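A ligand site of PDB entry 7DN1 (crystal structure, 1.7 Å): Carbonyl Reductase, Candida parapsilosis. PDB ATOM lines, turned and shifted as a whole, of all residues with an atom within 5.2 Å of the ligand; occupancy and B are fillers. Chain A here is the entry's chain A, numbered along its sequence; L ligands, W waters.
O13 of the ligand sits at hydrogen-bond distance from OH of Tyr 188 (2.6 Å). N3 of the ligand lies within hydrogen-bond range of OD1 of Asn 92, at 2.7 Å. An oxygen (O15) of the ligand is in hydrogen-bond range of the backbone NH of Ser 68 (2.8 Å). OG of Ser 68 is in hydrogen-bond range of O15 of the ligand, 2.7 Å away. OG of Ser 44 sits at hydrogen-bond distance from O5 of the ligand, at 2.7 Å. The backbone carbonyl oxygen (O) of Asn 119 is in hydrogen-bond range of an oxygen (O12) of the ligand, 2.7 Å away. An oxygen (O9) of the ligand lies within hydrogen-bond range of the side-chain hydroxyl (OG1) of Thr 222 (2.8 Å). The backbone NH of His 69 sits at hydrogen-bond distance from an oxygen (O16) of the ligand, at 3.0 Å. ND1 of His 69 is in hydrogen-bond range of O17 of the ligand, 2.9 Å away. N of Asn 67 is in hydrogen-bond range of O16 of the ligand, 3.0 Å away. The backbone NH of Ile 220 is in hydrogen-bond range of an oxygen (O14) of the ligand. The backbone NH (N) of Ile 47 lies within hydrogen-bond range of an oxygen (O8) of the ligand, at 3.0 Å. The side-chain amino group (NZ) of Lys 192 sits at hydrogen-bond distance from an oxygen (O12) of the ligand (3.0 Å). N of Gly 46 sits at hydrogen-bond distance from O1 of the ligand. An oxygen (O5) of the ligand is in hydrogen-bond range of the backbone NH (N) of Gly 45. N of Ile 93 sits at hydrogen-bond distance from N4 of the ligand, 3.1 Å away. The backbone carbonyl oxygen (O) of Gly 42 sits close to an oxygen (O5) of the ligand, at 3.2 Å. N of Gly 121 lies within hydrogen-bond range of O4 of the ligand.
Water W2 bridges O2 of the ligand (2.7 Å) and O of Gly 121 (3.0 Å). Water W4 lies within hydrogen-bond range of O8 of the ligand (2.7 Å), N of Gly 48 (2.8 Å), O of Gly 42 (2.8 Å), OD1 of Asn 119 (2.9 Å) and N of Ile 47 (3.5 Å). Water W1 lies within hydrogen-bond range of N of Gly 42 (2.9 Å) and N5 of the ligand (3.0 Å).
OG1 of Thr 171 sits at hydrogen-bond distance from ND2 of Asn 119 (2.8 Å). The side-chain hydroxyl (OG1) of Thr 222 sits close to the backbone NH (N) of Ile 224 (3.3 Å). The backbone carbonyl oxygen (O) of Thr 222 sits at hydrogen-bond distance from the side-chain hydroxyl (OG1) of Thr 225, 3.4 Å away. O of Lys 192 is in hydrogen-bond range of OG of Ser 172, 3.0 Å away. The backbone NH of Cys 91 sits at hydrogen-bond distance from the backbone carbonyl oxygen of Tyr 66 (3.0 Å). O of Pro 217 is in hydrogen-bond range of N of Ile 174, 3.0 Å away. The side-chain hydroxyl (OG) of Ser 43 lies within hydrogen-bond range of the backbone carbonyl oxygen (O) of Gly 48, 3.4 Å away. The backbone NH of Ser 43 is in hydrogen-bond range of the backbone carbonyl oxygen of Trp 65 (3.0 Å).
Ser 43 touches the ligand (N to O5, 3.9 Å). Tyr 66 touches the ligand. O of Cys 91 touches C9 of the ligand, 3.1 Å away. Ala 120 touches the ligand. Val 122 touches the ligand (CG1 to N2, 3.6 Å). Thr 171 touches the ligand. O of Ser 172 touches C21 of the ligand (3.3 Å). Ser 173 touches the ligand (OG to C20, 3.4 Å). O of Pro 217 touches C20 of the ligand, at 3.2 Å. Gly 218 touches the ligand (O to C19, 2.8 Å). Tyr 219 touches the ligand. Ile 224 touches the ligand (CG2 to N7, 3.2 Å). CG2 of Thr 225 touches O14 of the ligand, at 3.9 Å. Hydrophobic or aromatic side chains that line the ligand: Ile 47, Tyr 66, His 69, Ile 93, Ala 120, Val 122, Tyr 188, Pro 217, Ile 220 and Ile 224. Within 4 Å of the ligand: Gly 42, Ser 43, Ser 44, Gly 45, Gly 46, Ile 47, Tyr 66, Asn 67, Ser 68, His 69, Cys 91, Asn 92, Ile 93, Asn 119, Ala 120, Gly 121, Val 122, Thr 171, Ser 172, Ser 173, Tyr 188, Lys 192, Pro 217, Gly 218, Tyr 219, Ile 220, Thr 222, Ile 224 and Thr 225.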
ATOM      1  N   GLY A  42      -4.111 -33.779  -6.689  1.00  0.00           N
ATOM      2  CA  GLY A  42      -3.907 -32.340  -6.716  1.00  0.00           C
ATOM      3  C   GLY A  42      -4.702 -31.666  -7.816  1.00  0.00           C
ATOM      4  O   GLY A  42      -4.245 -30.686  -8.408  1.00  0.00           O
ATOM      5  N   SER A  43      -5.899 -32.164  -8.077  1.00  0.00           N
ATOM      6  CA  SER A  43      -6.653 -31.792  -9.254  1.00  0.00           C
ATOM      7  C   SER A  43      -7.651 -30.669  -8.930  1.00  0.00           C
ATOM      8  O   SER A  43      -8.376 -30.202  -9.823  1.00  0.00           O
ATOM      9  CB  SER A  43      -7.314 -33.044  -9.831  1.00  0.00           C
ATOM     10  OG  SER A  43      -8.087 -32.777 -10.977  1.00  0.00           O
ATOM     11  N   SER A  44      -7.684 -30.232  -7.675  1.00  0.00           N
ATOM     12  CA  SER A  44      -8.269 -28.938  -7.346  1.00  0.00           C
ATOM     13  C   SER A  44      -7.342 -27.786  -7.692  1.00  0.00           C
ATOM     14  O   SER A  44      -7.772 -26.623  -7.655  1.00  0.00           O
ATOM     15  CB  SER A  44      -8.629 -28.891  -5.856  1.00  0.00           C
ATOM     16  OG  SER A  44      -7.486 -29.117  -5.041  1.00  0.00           O
ATOM     17  N   GLY A  45      -6.077 -28.071  -8.019  1.00  0.00           N
ATOM     18  CA  GLY A  45      -5.107 -27.042  -8.319  1.00  0.00           C
ATOM     19  C   GLY A  45      -4.911 -26.828  -9.818  1.00  0.00           C
ATOM     20  O   GLY A  45      -5.550 -27.448 -10.659  1.00  0.00           O
ATOM     21  N   GLY A  46      -3.972 -25.931 -10.122  1.00  0.00           N
ATOM     22  CA  GLY A  46      -3.804 -25.412 -11.473  1.00  0.00           C
ATOM     23  C   GLY A  46      -3.438 -26.440 -12.516  1.00  0.00           C
ATOM     24  O   GLY A  46      -4.188 -26.674 -13.468  1.00  0.00           O
ATOM     25  N   ILE A  47      -2.267 -27.064 -12.342  1.00  0.00           N
ATOM     26  CA  ILE A  47      -1.809 -28.075 -13.288  1.00  0.00           C
ATOM     27  C   ILE A  47      -2.735 -29.285 -13.274  1.00  0.00           C
ATOM     28  O   ILE A  47      -3.108 -29.804 -14.324  1.00  0.00           O
ATOM     29  CB  ILE A  47      -0.351 -28.450 -12.975  1.00  0.00           C
ATOM     30  CG1 ILE A  47       0.557 -27.207 -13.127  1.00  0.00           C
ATOM     31  CG2 ILE A  47       0.090 -29.663 -13.817  1.00  0.00           C
ATOM     32  CD1 ILE A  47       2.034 -27.460 -12.808  1.00  0.00           C
ATOM     33  N   GLY A  48      -3.147 -29.726 -12.081  1.00  0.00           N
ATOM     34  CA  GLY A  48      -3.961 -30.936 -11.982  1.00  0.00           C
ATOM     35  C   GLY A  48      -5.310 -30.797 -12.680  1.00  0.00           C
ATOM     36  O   GLY A  48      -5.789 -31.737 -13.321  1.00  0.00           O
ATOM     37  N   TRP A  65      -8.931 -35.269  -7.210  1.00  0.00           N
ATOM     38  CA  TRP A  65      -8.497 -35.263  -5.823  1.00  0.00           C
ATOM     39  C   TRP A  65      -8.398 -33.834  -5.320  1.00  0.00           C
ATOM     40  O   TRP A  65      -7.952 -32.943  -6.040  1.00  0.00           O
ATOM     41  CB  TRP A  65      -7.136 -35.907  -5.613  1.00  0.00           C
ATOM     42  CG  TRP A  65      -6.973 -37.356  -6.022  1.00  0.00           C
ATOM     43  CD1 TRP A  65      -7.295 -37.916  -7.225  1.00  0.00           C
ATOM     44  CD2 TRP A  65      -6.412 -38.389  -5.235  1.00  0.00           C
ATOM     45  NE1 TRP A  65      -6.970 -39.252  -7.225  1.00  0.00           N
ATOM     46  CE2 TRP A  65      -6.423 -39.573  -6.005  1.00  0.00           C
ATOM     47  CE3 TRP A  65      -5.895 -38.448  -3.936  1.00  0.00           C
ATOM     48  CZ2 TRP A  65      -5.945 -40.784  -5.527  1.00  0.00           C
ATOM     49  CZ3 TRP A  65      -5.417 -39.659  -3.458  1.00  0.00           C
ATOM     50  CH2 TRP A  65      -5.445 -40.811  -4.258  1.00  0.00           C
ATOM     51  N   TYR A  66      -8.777 -33.635  -4.059  1.00  0.00           N
ATOM     52  CA  TYR A  66      -8.583 -32.345  -3.407  1.00  0.00           C
ATOM     53  C   TYR A  66      -8.281 -32.598  -1.940  1.00  0.00           C
ATOM     54  O   TYR A  66      -8.482 -33.692  -1.428  1.00  0.00           O
ATOM     55  CB  TYR A  66      -9.809 -31.439  -3.611  1.00  0.00           C
ATOM     56  CG  TYR A  66     -11.081 -31.933  -2.947  1.00  0.00           C
ATOM     57  CD1 TYR A  66     -11.289 -31.782  -1.582  1.00  0.00           C
ATOM     58  CD2 TYR A  66     -12.033 -32.627  -3.690  1.00  0.00           C
ATOM     59  CE1 TYR A  66     -12.452 -32.252  -0.977  1.00  0.00           C
ATOM     60  CE2 TYR A  66     -13.185 -33.104  -3.102  1.00  0.00           C
ATOM     61  CZ  TYR A  66     -13.384 -32.920  -1.751  1.00  0.00           C
ATOM     62  OH  TYR A  66     -14.544 -33.398  -1.168  1.00  0.00           O
ATOM     63  N   ASN A  67      -7.789 -31.560  -1.264  1.00  0.00           N
ATOM     64  CA  ASN A  67      -7.553 -31.644   0.173  1.00  0.00           C
ATOM     65  C   ASN A  67      -8.309 -30.545   0.914  1.00  0.00           C
ATOM     66  O   ASN A  67      -9.289 -30.848   1.603  1.00  0.00           O
ATOM     67  CB  ASN A  67      -6.059 -31.572   0.479  1.00  0.00           C
ATOM     68  CG  ASN A  67      -5.748 -31.874   1.933  1.00  0.00           C
ATOM     69  OD1 ASN A  67      -6.423 -32.682   2.564  1.00  0.00           O
ATOM     70  ND2 ASN A  67      -4.724 -31.225   2.475  1.00  0.00           N
ATOM     71  N   SER A  68      -7.888 -29.292   0.796  1.00  0.00           N
ATOM     72  CA  SER A  68      -8.508 -28.192   1.530  1.00  0.00           C
ATOM     73  C   SER A  68      -9.471 -27.373   0.667  1.00  0.00           C
ATOM     74  O   SER A  68     -10.169 -26.510   1.194  1.00  0.00           O
ATOM     75  CB  SER A  68      -7.429 -27.282   2.111  1.00  0.00           C
ATOM     76  OG  SER A  68      -6.737 -26.584   1.089  1.00  0.00           O
ATOM     77  N   HIS A  69      -9.529 -27.641  -0.635  1.00  0.00           N
ATOM     78  CA  HIS A  69     -10.488 -26.981  -1.519  1.00  0.00           C
ATOM     79  C   HIS A  69     -11.337 -28.012  -2.233  1.00  0.00           C
ATOM     80  O   HIS A  69     -10.908 -28.575  -3.251  1.00  0.00           O
ATOM     81  CB  HIS A  69      -9.772 -26.100  -2.546  1.00  0.00           C
ATOM     82  CG  HIS A  69      -8.993 -24.972  -1.947  1.00  0.00           C
ATOM     83  ND1 HIS A  69      -7.640 -25.066  -1.697  1.00  0.00           N
ATOM     84  CD2 HIS A  69      -9.372 -23.742  -1.530  1.00  0.00           C
ATOM     85  CE1 HIS A  69      -7.210 -23.928  -1.166  1.00  0.00           C
ATOM     86  NE2 HIS A  69      -8.245 -23.110  -1.055  1.00  0.00           N
ATOM     87  N   CYS A  91      -8.514 -36.176   0.334  1.00  0.00           N
ATOM     88  CA  CYS A  91      -7.462 -36.982   0.932  1.00  0.00           C
ATOM     89  C   CYS A  91      -6.251 -36.117   1.256  1.00  0.00           C
ATOM     90  O   CYS A  91      -5.805 -35.316   0.426  1.00  0.00           O
ATOM     91  CB  CYS A  91      -7.033 -38.127  -0.004  1.00  0.00           C
ATOM     92  SG  CYS A  91      -5.732 -39.174   0.672  1.00  0.00           S
ATOM     93  N   ASN A  92      -5.727 -36.279   2.472  1.00  0.00           N
ATOM     94  CA  ASN A  92      -4.406 -35.770   2.815  1.00  0.00           C
ATOM     95  C   ASN A  92      -3.396 -36.835   2.435  1.00  0.00           C
ATOM     96  O   ASN A  92      -3.278 -37.871   3.115  1.00  0.00           O
ATOM     97  CB  ASN A  92      -4.319 -35.416   4.292  1.00  0.00           C
ATOM     98  CG  ASN A  92      -2.915 -34.999   4.711  1.00  0.00           C
ATOM     99  OD1 ASN A  92      -2.061 -34.690   3.868  1.00  0.00           O
ATOM    100  ND2 ASN A  92      -2.672 -35.008   6.007  1.00  0.00           N
ATOM    101  N   ILE A  93      -2.675 -36.602   1.339  1.00  0.00           N
ATOM    102  CA  ILE A  93      -1.702 -37.566   0.830  1.00  0.00           C
ATOM    103  C   ILE A  93      -0.499 -37.777   1.735  1.00  0.00           C
ATOM    104  O   ILE A  93       0.244 -38.750   1.544  1.00  0.00           O
ATOM    105  CB  ILE A  93      -1.389 -37.146  -0.633  1.00  0.00           C
ATOM    106  CG1 ILE A  93      -2.682 -37.282  -1.467  1.00  0.00           C
ATOM    107  CG2 ILE A  93      -0.138 -37.789  -1.227  1.00  0.00           C
ATOM    108  CD1 ILE A  93      -2.620 -36.688  -2.840  1.00  0.00           C
ATOM    109  N   SER A  94      -0.287 -36.935   2.753  1.00  0.00           N
ATOM    110  CA  SER A  94       0.721 -37.269   3.741  1.00  0.00           C
ATOM    111  C   SER A  94       0.310 -38.453   4.596  1.00  0.00           C
ATOM    112  O   SER A  94       1.167 -39.039   5.269  1.00  0.00           O
ATOM    113  CB  SER A  94       1.038 -36.063   4.628  1.00  0.00           C
ATOM    114  OG  SER A  94       1.829 -35.146   3.908  1.00  0.00           O
ATOM    115  N   ASN A 119       0.502 -35.780  -8.619  1.00  0.00           N
ATOM    116  CA  ASN A 119       0.701 -34.380  -8.967  1.00  0.00           C
ATOM    117  C   ASN A 119       0.598 -33.427  -7.777  1.00  0.00           C
ATOM    118  O   ASN A 119       1.220 -32.369  -7.818  1.00  0.00           O
ATOM    119  CB  ASN A 119      -0.331 -33.988 -10.046  1.00  0.00           C
ATOM    120  CG  ASN A 119      -0.428 -32.492 -10.272  1.00  0.00           C
ATOM    121  OD1 ASN A 119      -1.403 -31.870  -9.864  1.00  0.00           O
ATOM    122  ND2 ASN A 119       0.560 -31.918 -10.940  1.00  0.00           N
ATOM    123  N   ALA A 120      -0.137 -33.778  -6.732  1.00  0.00           N
ATOM    124  CA  ALA A 120      -0.277 -32.895  -5.576  1.00  0.00           C
ATOM    125  C   ALA A 120       1.088 -32.560  -4.966  1.00  0.00           C
ATOM    126  O   ALA A 120       1.981 -33.397  -4.896  1.00  0.00           O
ATOM    127  CB  ALA A 120      -1.170 -33.540  -4.521  1.00  0.00           C
ATOM    128  N   GLY A 121       1.231 -31.315  -4.510  1.00  0.00           N
ATOM    129  CA  GLY A 121       2.499 -30.915  -3.917  1.00  0.00           C
ATOM    130  C   GLY A 121       2.399 -29.532  -3.309  1.00  0.00           C
ATOM    131  O   GLY A 121       1.457 -28.770  -3.579  1.00  0.00           O
ATOM    132  N   VAL A 122       3.382 -29.220  -2.459  1.00  0.00           N
ATOM    133  CA  VAL A 122       3.493 -27.902  -1.844  1.00  0.00           C
ATOM    134  C   VAL A 122       4.909 -27.385  -2.015  1.00  0.00           C
ATOM    135  O   VAL A 122       5.882 -28.141  -2.085  1.00  0.00           O
ATOM    136  CB  VAL A 122       3.096 -27.918  -0.351  1.00  0.00           C
ATOM    137  CG1 VAL A 122       1.618 -28.216  -0.200  1.00  0.00           C
ATOM    138  CG2 VAL A 122       3.933 -28.957   0.398  1.00  0.00           C
ATOM    139  N   THR A 123       5.042 -26.061  -2.058  1.00  0.00           N
ATOM    140  CA  THR A 123       6.351 -25.447  -2.175  1.00  0.00           C
ATOM    141  C   THR A 123       6.952 -25.061  -0.829  1.00  0.00           C
ATOM    142  O   THR A 123       6.266 -24.921   0.188  1.00  0.00           O
ATOM    143  CB  THR A 123       6.267 -24.195  -3.077  1.00  0.00           C
ATOM    144  OG1 THR A 123       5.352 -23.252  -2.510  1.00  0.00           O
ATOM    145  CG2 THR A 123       5.997 -24.545  -4.528  1.00  0.00           C
ATOM    146  N   VAL A 144       4.831 -34.648   1.976  1.00  0.00           N
ATOM    147  CA  VAL A 144       3.862 -34.473   0.894  1.00  0.00           C
ATOM    148  C   VAL A 144       4.483 -34.746  -0.461  1.00  0.00           C
ATOM    149  O   VAL A 144       3.940 -35.491  -1.283  1.00  0.00           O
ATOM    150  CB  VAL A 144       3.270 -33.051   0.937  1.00  0.00           C
ATOM    151  CG1 VAL A 144       2.315 -32.845  -0.240  1.00  0.00           C
ATOM    152  CG2 VAL A 144       2.617 -32.718   2.267  1.00  0.00           C
ATOM    153  N   THR A 171       4.375 -35.757 -11.498  1.00  0.00           N
ATOM    154  CA  THR A 171       4.756 -34.358 -11.705  1.00  0.00           C
ATOM    155  C   THR A 171       5.982 -34.069 -10.844  1.00  0.00           C
ATOM    156  O   THR A 171       5.885 -33.996  -9.611  1.00  0.00           O
ATOM    157  CB  THR A 171       3.641 -33.379 -11.345  1.00  0.00           C
ATOM    158  OG1 THR A 171       2.466 -33.665 -12.101  1.00  0.00           O
ATOM    159  CG2 THR A 171       4.098 -31.924 -11.651  1.00  0.00           C
ATOM    160  N   SER A 172       7.130 -33.950 -11.475  1.00  0.00           N
ATOM    161  CA  SER A 172       8.347 -33.522 -10.804  1.00  0.00           C
ATOM    162  C   SER A 172       8.494 -32.010 -11.001  1.00  0.00           C
ATOM    163  O   SER A 172       7.502 -31.308 -10.808  1.00  0.00           O
ATOM    164  CB  SER A 172       9.531 -34.333 -11.273  1.00  0.00           C
ATOM    165  OG  SER A 172      10.668 -34.004 -10.477  1.00  0.00           O
ATOM    166  N   SER A 173       9.637 -31.500 -11.411  1.00  0.00           N
ATOM    167  CA  SER A 173       9.852 -30.068 -11.564  1.00  0.00           C
ATOM    168  C   SER A 173      11.234 -29.924 -12.172  1.00  0.00           C
ATOM    169  O   SER A 173      12.064 -30.824 -12.020  1.00  0.00           O
ATOM    170  CB  SER A 173       9.780 -29.340 -10.218  1.00  0.00           C
ATOM    171  OG  SER A 173      10.269 -28.022 -10.331  1.00  0.00           O
ATOM    172  N   ILE A 174      11.482 -28.792 -12.829  1.00  0.00           N
ATOM    173  CA  ILE A 174      12.873 -28.504 -13.158  1.00  0.00           C
ATOM    174  C   ILE A 174      13.709 -28.415 -11.895  1.00  0.00           C
ATOM    175  O   ILE A 174      14.917 -28.580 -11.953  1.00  0.00           O
ATOM    176  CB  ILE A 174      13.032 -27.236 -14.032  1.00  0.00           C
ATOM    177  CG1 ILE A 174      12.425 -25.983 -13.411  1.00  0.00           C
ATOM    178  CG2 ILE A 174      12.459 -27.465 -15.421  1.00  0.00           C
ATOM    179  CD1 ILE A 174      12.803 -24.723 -14.253  1.00  0.00           C
ATOM    180  N   TYR A 188      12.676 -28.506  -1.268  1.00  0.00           N
ATOM    181  CA  TYR A 188      11.806 -28.792  -2.402  1.00  0.00           C
ATOM    182  C   TYR A 188      12.605 -29.383  -3.568  1.00  0.00           C
ATOM    183  O   TYR A 188      12.183 -30.373  -4.168  1.00  0.00           O
ATOM    184  CB  TYR A 188      11.087 -27.515  -2.823  1.00  0.00           C
ATOM    185  CG  TYR A 188      10.187 -27.635  -4.024  1.00  0.00           C
ATOM    186  CD1 TYR A 188      10.655 -27.353  -5.300  1.00  0.00           C
ATOM    187  CD2 TYR A 188       8.843 -27.973  -3.876  1.00  0.00           C
ATOM    188  CE1 TYR A 188       9.813 -27.417  -6.407  1.00  0.00           C
ATOM    189  CE2 TYR A 188       7.988 -28.049  -4.981  1.00  0.00           C
ATOM    190  CZ  TYR A 188       8.490 -27.776  -6.237  1.00  0.00           C
ATOM    191  OH  TYR A 188       7.664 -27.840  -7.333  1.00  0.00           O
ATOM    192  N   LYS A 192      12.001 -33.143  -5.236  1.00  0.00           N
ATOM    193  CA  LYS A 192      11.697 -33.307  -6.657  1.00  0.00           C
ATOM    194  C   LYS A 192      12.763 -34.122  -7.384  1.00  0.00           C
ATOM    195  O   LYS A 192      12.443 -34.925  -8.274  1.00  0.00           O
ATOM    196  CB  LYS A 192      11.501 -31.937  -7.314  1.00  0.00           C
ATOM    197  CG  LYS A 192      10.193 -31.259  -6.909  1.00  0.00           C
ATOM    198  CD  LYS A 192       8.970 -32.091  -7.380  1.00  0.00           C
ATOM    199  CE  LYS A 192       7.671 -31.304  -7.156  1.00  0.00           C
ATOM    200  NZ  LYS A 192       6.448 -32.142  -7.352  1.00  0.00           N
ATOM    201  N   PRO A 217       7.806 -29.630 -15.105  1.00  0.00           N
ATOM    202  CA  PRO A 217       7.482 -28.277 -15.584  1.00  0.00           C
ATOM    203  C   PRO A 217       8.529 -27.264 -15.139  1.00  0.00           C
ATOM    204  O   PRO A 217       9.176 -27.410 -14.094  1.00  0.00           O
ATOM    205  CB  PRO A 217       6.120 -27.969 -14.943  1.00  0.00           C
ATOM    206  CG  PRO A 217       5.587 -29.312 -14.503  1.00  0.00           C
ATOM    207  CD  PRO A 217       6.814 -30.113 -14.138  1.00  0.00           C
ATOM    208  N   GLY A 218       8.652 -26.189 -15.934  1.00  0.00           N
ATOM    209  CA  GLY A 218       9.334 -24.980 -15.517  1.00  0.00           C
ATOM    210  C   GLY A 218       8.409 -24.101 -14.714  1.00  0.00           C
ATOM    211  O   GLY A 218       7.540 -24.581 -13.991  1.00  0.00           O
ATOM    212  N   TYR A 219       8.600 -22.785 -14.828  1.00  0.00           N
ATOM    213  CA  TYR A 219       7.735 -21.829 -14.155  1.00  0.00           C
ATOM    214  C   TYR A 219       6.402 -21.725 -14.895  1.00  0.00           C
ATOM    215  O   TYR A 219       6.366 -21.282 -16.041  1.00  0.00           O
ATOM    216  CB  TYR A 219       8.419 -20.465 -14.075  1.00  0.00           C
ATOM    217  CG  TYR A 219       9.593 -20.472 -13.111  1.00  0.00           C
ATOM    218  CD1 TYR A 219       9.386 -20.613 -11.741  1.00  0.00           C
ATOM    219  CD2 TYR A 219      10.907 -20.348 -13.574  1.00  0.00           C
ATOM    220  CE1 TYR A 219      10.453 -20.641 -10.850  1.00  0.00           C
ATOM    221  CE2 TYR A 219      11.981 -20.366 -12.677  1.00  0.00           C
ATOM    222  CZ  TYR A 219      11.735 -20.518 -11.322  1.00  0.00           C
ATOM    223  OH  TYR A 219      12.769 -20.540 -10.416  1.00  0.00           O
ATOM    224  N   ILE A 220       5.309 -22.125 -14.233  1.00  0.00           N
ATOM    225  CA  ILE A 220       3.970 -22.148 -14.815  1.00  0.00           C
ATOM    226  C   ILE A 220       3.104 -21.172 -14.031  1.00  0.00           C
ATOM    227  O   ILE A 220       3.209 -21.085 -12.798  1.00  0.00           O
ATOM    228  CB  ILE A 220       3.367 -23.574 -14.817  1.00  0.00           C
ATOM    229  CG1 ILE A 220       4.332 -24.600 -15.423  1.00  0.00           C
ATOM    230  CG2 ILE A 220       2.028 -23.619 -15.582  1.00  0.00           C
ATOM    231  CD1 ILE A 220       4.644 -24.410 -16.898  1.00  0.00           C
ATOM    232  N   THR A 222       0.571 -20.406 -12.089  1.00  0.00           N
ATOM    233  CA  THR A 222      -0.442 -20.878 -11.146  1.00  0.00           C
ATOM    234  C   THR A 222      -0.275 -20.097  -9.855  1.00  0.00           C
ATOM    235  O   THR A 222       0.585 -19.217  -9.744  1.00  0.00           O
ATOM    236  CB  THR A 222      -0.330 -22.387 -10.889  1.00  0.00           C
ATOM    237  OG1 THR A 222       0.850 -22.665 -10.130  1.00  0.00           O
ATOM    238  CG2 THR A 222      -0.273 -23.170 -12.192  1.00  0.00           C
ATOM    239  N   ASP A 223      -1.110 -20.409  -8.857  1.00  0.00           N
ATOM    240  CA  ASP A 223      -1.023 -19.724  -7.571  1.00  0.00           C
ATOM    241  C   ASP A 223       0.122 -20.228  -6.699  1.00  0.00           C
ATOM    242  O   ASP A 223       0.387 -19.637  -5.648  1.00  0.00           O
ATOM    243  CB  ASP A 223      -2.340 -19.838  -6.808  1.00  0.00           C
ATOM    244  CG  ASP A 223      -3.520 -19.334  -7.606  1.00  0.00           C
ATOM    245  OD1 ASP A 223      -4.678 -19.497  -7.143  1.00  0.00           O
ATOM    246  OD2 ASP A 223      -3.302 -18.786  -8.704  1.00  0.00           O
ATOM    247  N   ILE A 224       0.811 -21.293  -7.119  1.00  0.00           N
ATOM    248  CA  ILE A 224       1.914 -21.833  -6.328  1.00  0.00           C
ATOM    249  C   ILE A 224       3.070 -20.834  -6.272  1.00  0.00           C
ATOM    250  O   ILE A 224       3.867 -20.849  -5.314  1.00  0.00           O
ATOM    251  CB  ILE A 224       2.360 -23.194  -6.901  1.00  0.00           C
ATOM    252  CG1 ILE A 224       3.000 -24.057  -5.833  1.00  0.00           C
ATOM    253  CG2 ILE A 224       3.338 -23.017  -8.042  1.00  0.00           C
ATOM    254  CD1 ILE A 224       3.244 -25.494  -6.296  1.00  0.00           C
ATOM    255  N   THR A 225       3.177 -19.942  -7.260  1.00  0.00           N
ATOM    256  CA  THR A 225       4.280 -18.985  -7.340  1.00  0.00           C
ATOM    257  C   THR A 225       3.867 -17.571  -6.967  1.00  0.00           C
ATOM    258  O   THR A 225       4.558 -16.608  -7.313  1.00  0.00           O
ATOM    259  CB  THR A 225       4.885 -18.991  -8.750  1.00  0.00           C
ATOM    260  OG1 THR A 225       3.934 -18.485  -9.699  1.00  0.00           O
ATOM    261  CG2 THR A 225       5.325 -20.398  -9.165  1.00  0.00           C
HETATM  262  P1  LIG L   1      -1.413 -25.614  -6.797  1.00  0.00           P
HETATM  263  O1  LIG L   1      -2.404 -24.836  -7.671  1.00  0.00           O
HETATM  264  O2  LIG L   1      -1.238 -25.084  -5.404  1.00  0.00           O
HETATM  265  O3  LIG L   1      -1.933 -27.206  -6.684  1.00  0.00           O
HETATM  266  C1  LIG L   1      -1.664 -27.852  -5.453  1.00  0.00           C
HETATM  267  C2  LIG L   1      -2.560 -29.073  -5.301  1.00  0.00           C
HETATM  268  O4  LIG L   1      -1.852 -29.988  -4.173  1.00  0.00           O
HETATM  269  C3  LIG L   1      -3.742 -28.726  -4.827  1.00  0.00           C
HETATM  270  O5  LIG L   1      -4.824 -29.474  -5.518  1.00  0.00           O
HETATM  271  C4  LIG L   1      -3.731 -29.106  -3.315  1.00  0.00           C
HETATM  272  O6  LIG L   1      -4.959 -29.458  -2.830  1.00  0.00           O
HETATM  273  C5  LIG L   1      -2.847 -30.334  -3.369  1.00  0.00           C
HETATM  274  N1  LIG L   1      -2.375 -30.683  -2.034  1.00  0.00           N
HETATM  275  C6  LIG L   1      -1.622 -29.767  -1.447  1.00  0.00           C
HETATM  276  N2  LIG L   1      -1.314 -30.266  -0.241  1.00  0.00           N
HETATM  277  C7  LIG L   1      -1.892 -31.471  -0.120  1.00  0.00           C
HETATM  278  C8  LIG L   1      -1.905 -32.388   0.888  1.00  0.00           C
HETATM  279  N3  LIG L   1      -1.408 -32.687   2.258  1.00  0.00           N
HETATM  280  N4  LIG L   1      -2.576 -33.521   0.730  1.00  0.00           N
HETATM  281  C9  LIG L   1      -3.254 -33.772  -0.406  1.00  0.00           C
HETATM  282  N5  LIG L   1      -3.245 -32.886  -1.410  1.00  0.00           N
HETATM  283  C10 LIG L   1      -2.558 -31.733  -1.239  1.00  0.00           C
HETATM  284  O7  LIG L   1       0.067 -25.631  -7.533  1.00  0.00           O
HETATM  285  P2  LIG L   1       0.419 -26.370  -8.963  1.00  0.00           P
HETATM  286  O8  LIG L   1      -0.801 -26.800  -9.721  1.00  0.00           O
HETATM  287  O9  LIG L   1       1.258 -25.425  -9.829  1.00  0.00           O
HETATM  288  O10 LIG L   1       1.397 -27.651  -8.519  1.00  0.00           O
HETATM  289  C11 LIG L   1       0.961 -28.958  -8.670  1.00  0.00           C
HETATM  290  C12 LIG L   1       2.333 -29.779  -8.804  1.00  0.00           C
HETATM  291  O11 LIG L   1       3.192 -29.102  -9.900  1.00  0.00           O
HETATM  292  C13 LIG L   1       3.026 -29.733  -7.724  1.00  0.00           C
HETATM  293  O12 LIG L   1       3.605 -31.064  -7.473  1.00  0.00           O
HETATM  294  C14 LIG L   1       4.275 -28.710  -8.048  1.00  0.00           C
HETATM  295  O13 LIG L   1       5.366 -28.966  -7.079  1.00  0.00           O
HETATM  296  C15 LIG L   1       4.572 -29.024  -9.235  1.00  0.00           C
HETATM  297  N6  LIG L   1       5.245 -27.950  -9.997  1.00  0.00           N
HETATM  298  C16 LIG L   1       4.588 -26.722 -10.181  1.00  0.00           C
HETATM  299  C17 LIG L   1       5.171 -25.689 -11.115  1.00  0.00           C
HETATM  300  C18 LIG L   1       4.523 -24.354 -11.241  1.00  0.00           C
HETATM  301  O14 LIG L   1       5.209 -23.463 -11.578  1.00  0.00           O
HETATM  302  N7  LIG L   1       3.107 -24.206 -10.972  1.00  0.00           N
HETATM  303  C19 LIG L   1       6.592 -25.816 -11.702  1.00  0.00           C
HETATM  304  C20 LIG L   1       7.167 -27.255 -11.591  1.00  0.00           C
HETATM  305  C21 LIG L   1       6.534 -28.212 -10.545  1.00  0.00           C
HETATM  306  P3  LIG L   1      -5.930 -28.350  -2.034  1.00  0.00           P
HETATM  307  O15 LIG L   1      -5.582 -28.328  -0.569  1.00  0.00           O
HETATM  308  O16 LIG L   1      -7.333 -28.797  -2.253  1.00  0.00           O
HETATM  309  O17 LIG L   1      -5.720 -26.977  -2.620  1.00  0.00           O
HETATM  310  O   HOH W   1      -4.672 -33.859  -3.859  1.00  0.00           O
HETATM  311  O   HOH W   2       0.574 -25.946  -3.662  1.00  0.00           O
HETATM  312  O   HOH W   3      -0.308 -29.861   2.848  1.00  0.00           O
HETATM  313  O   HOH W   4      -2.232 -29.065  -9.517  1.00  0.00           O
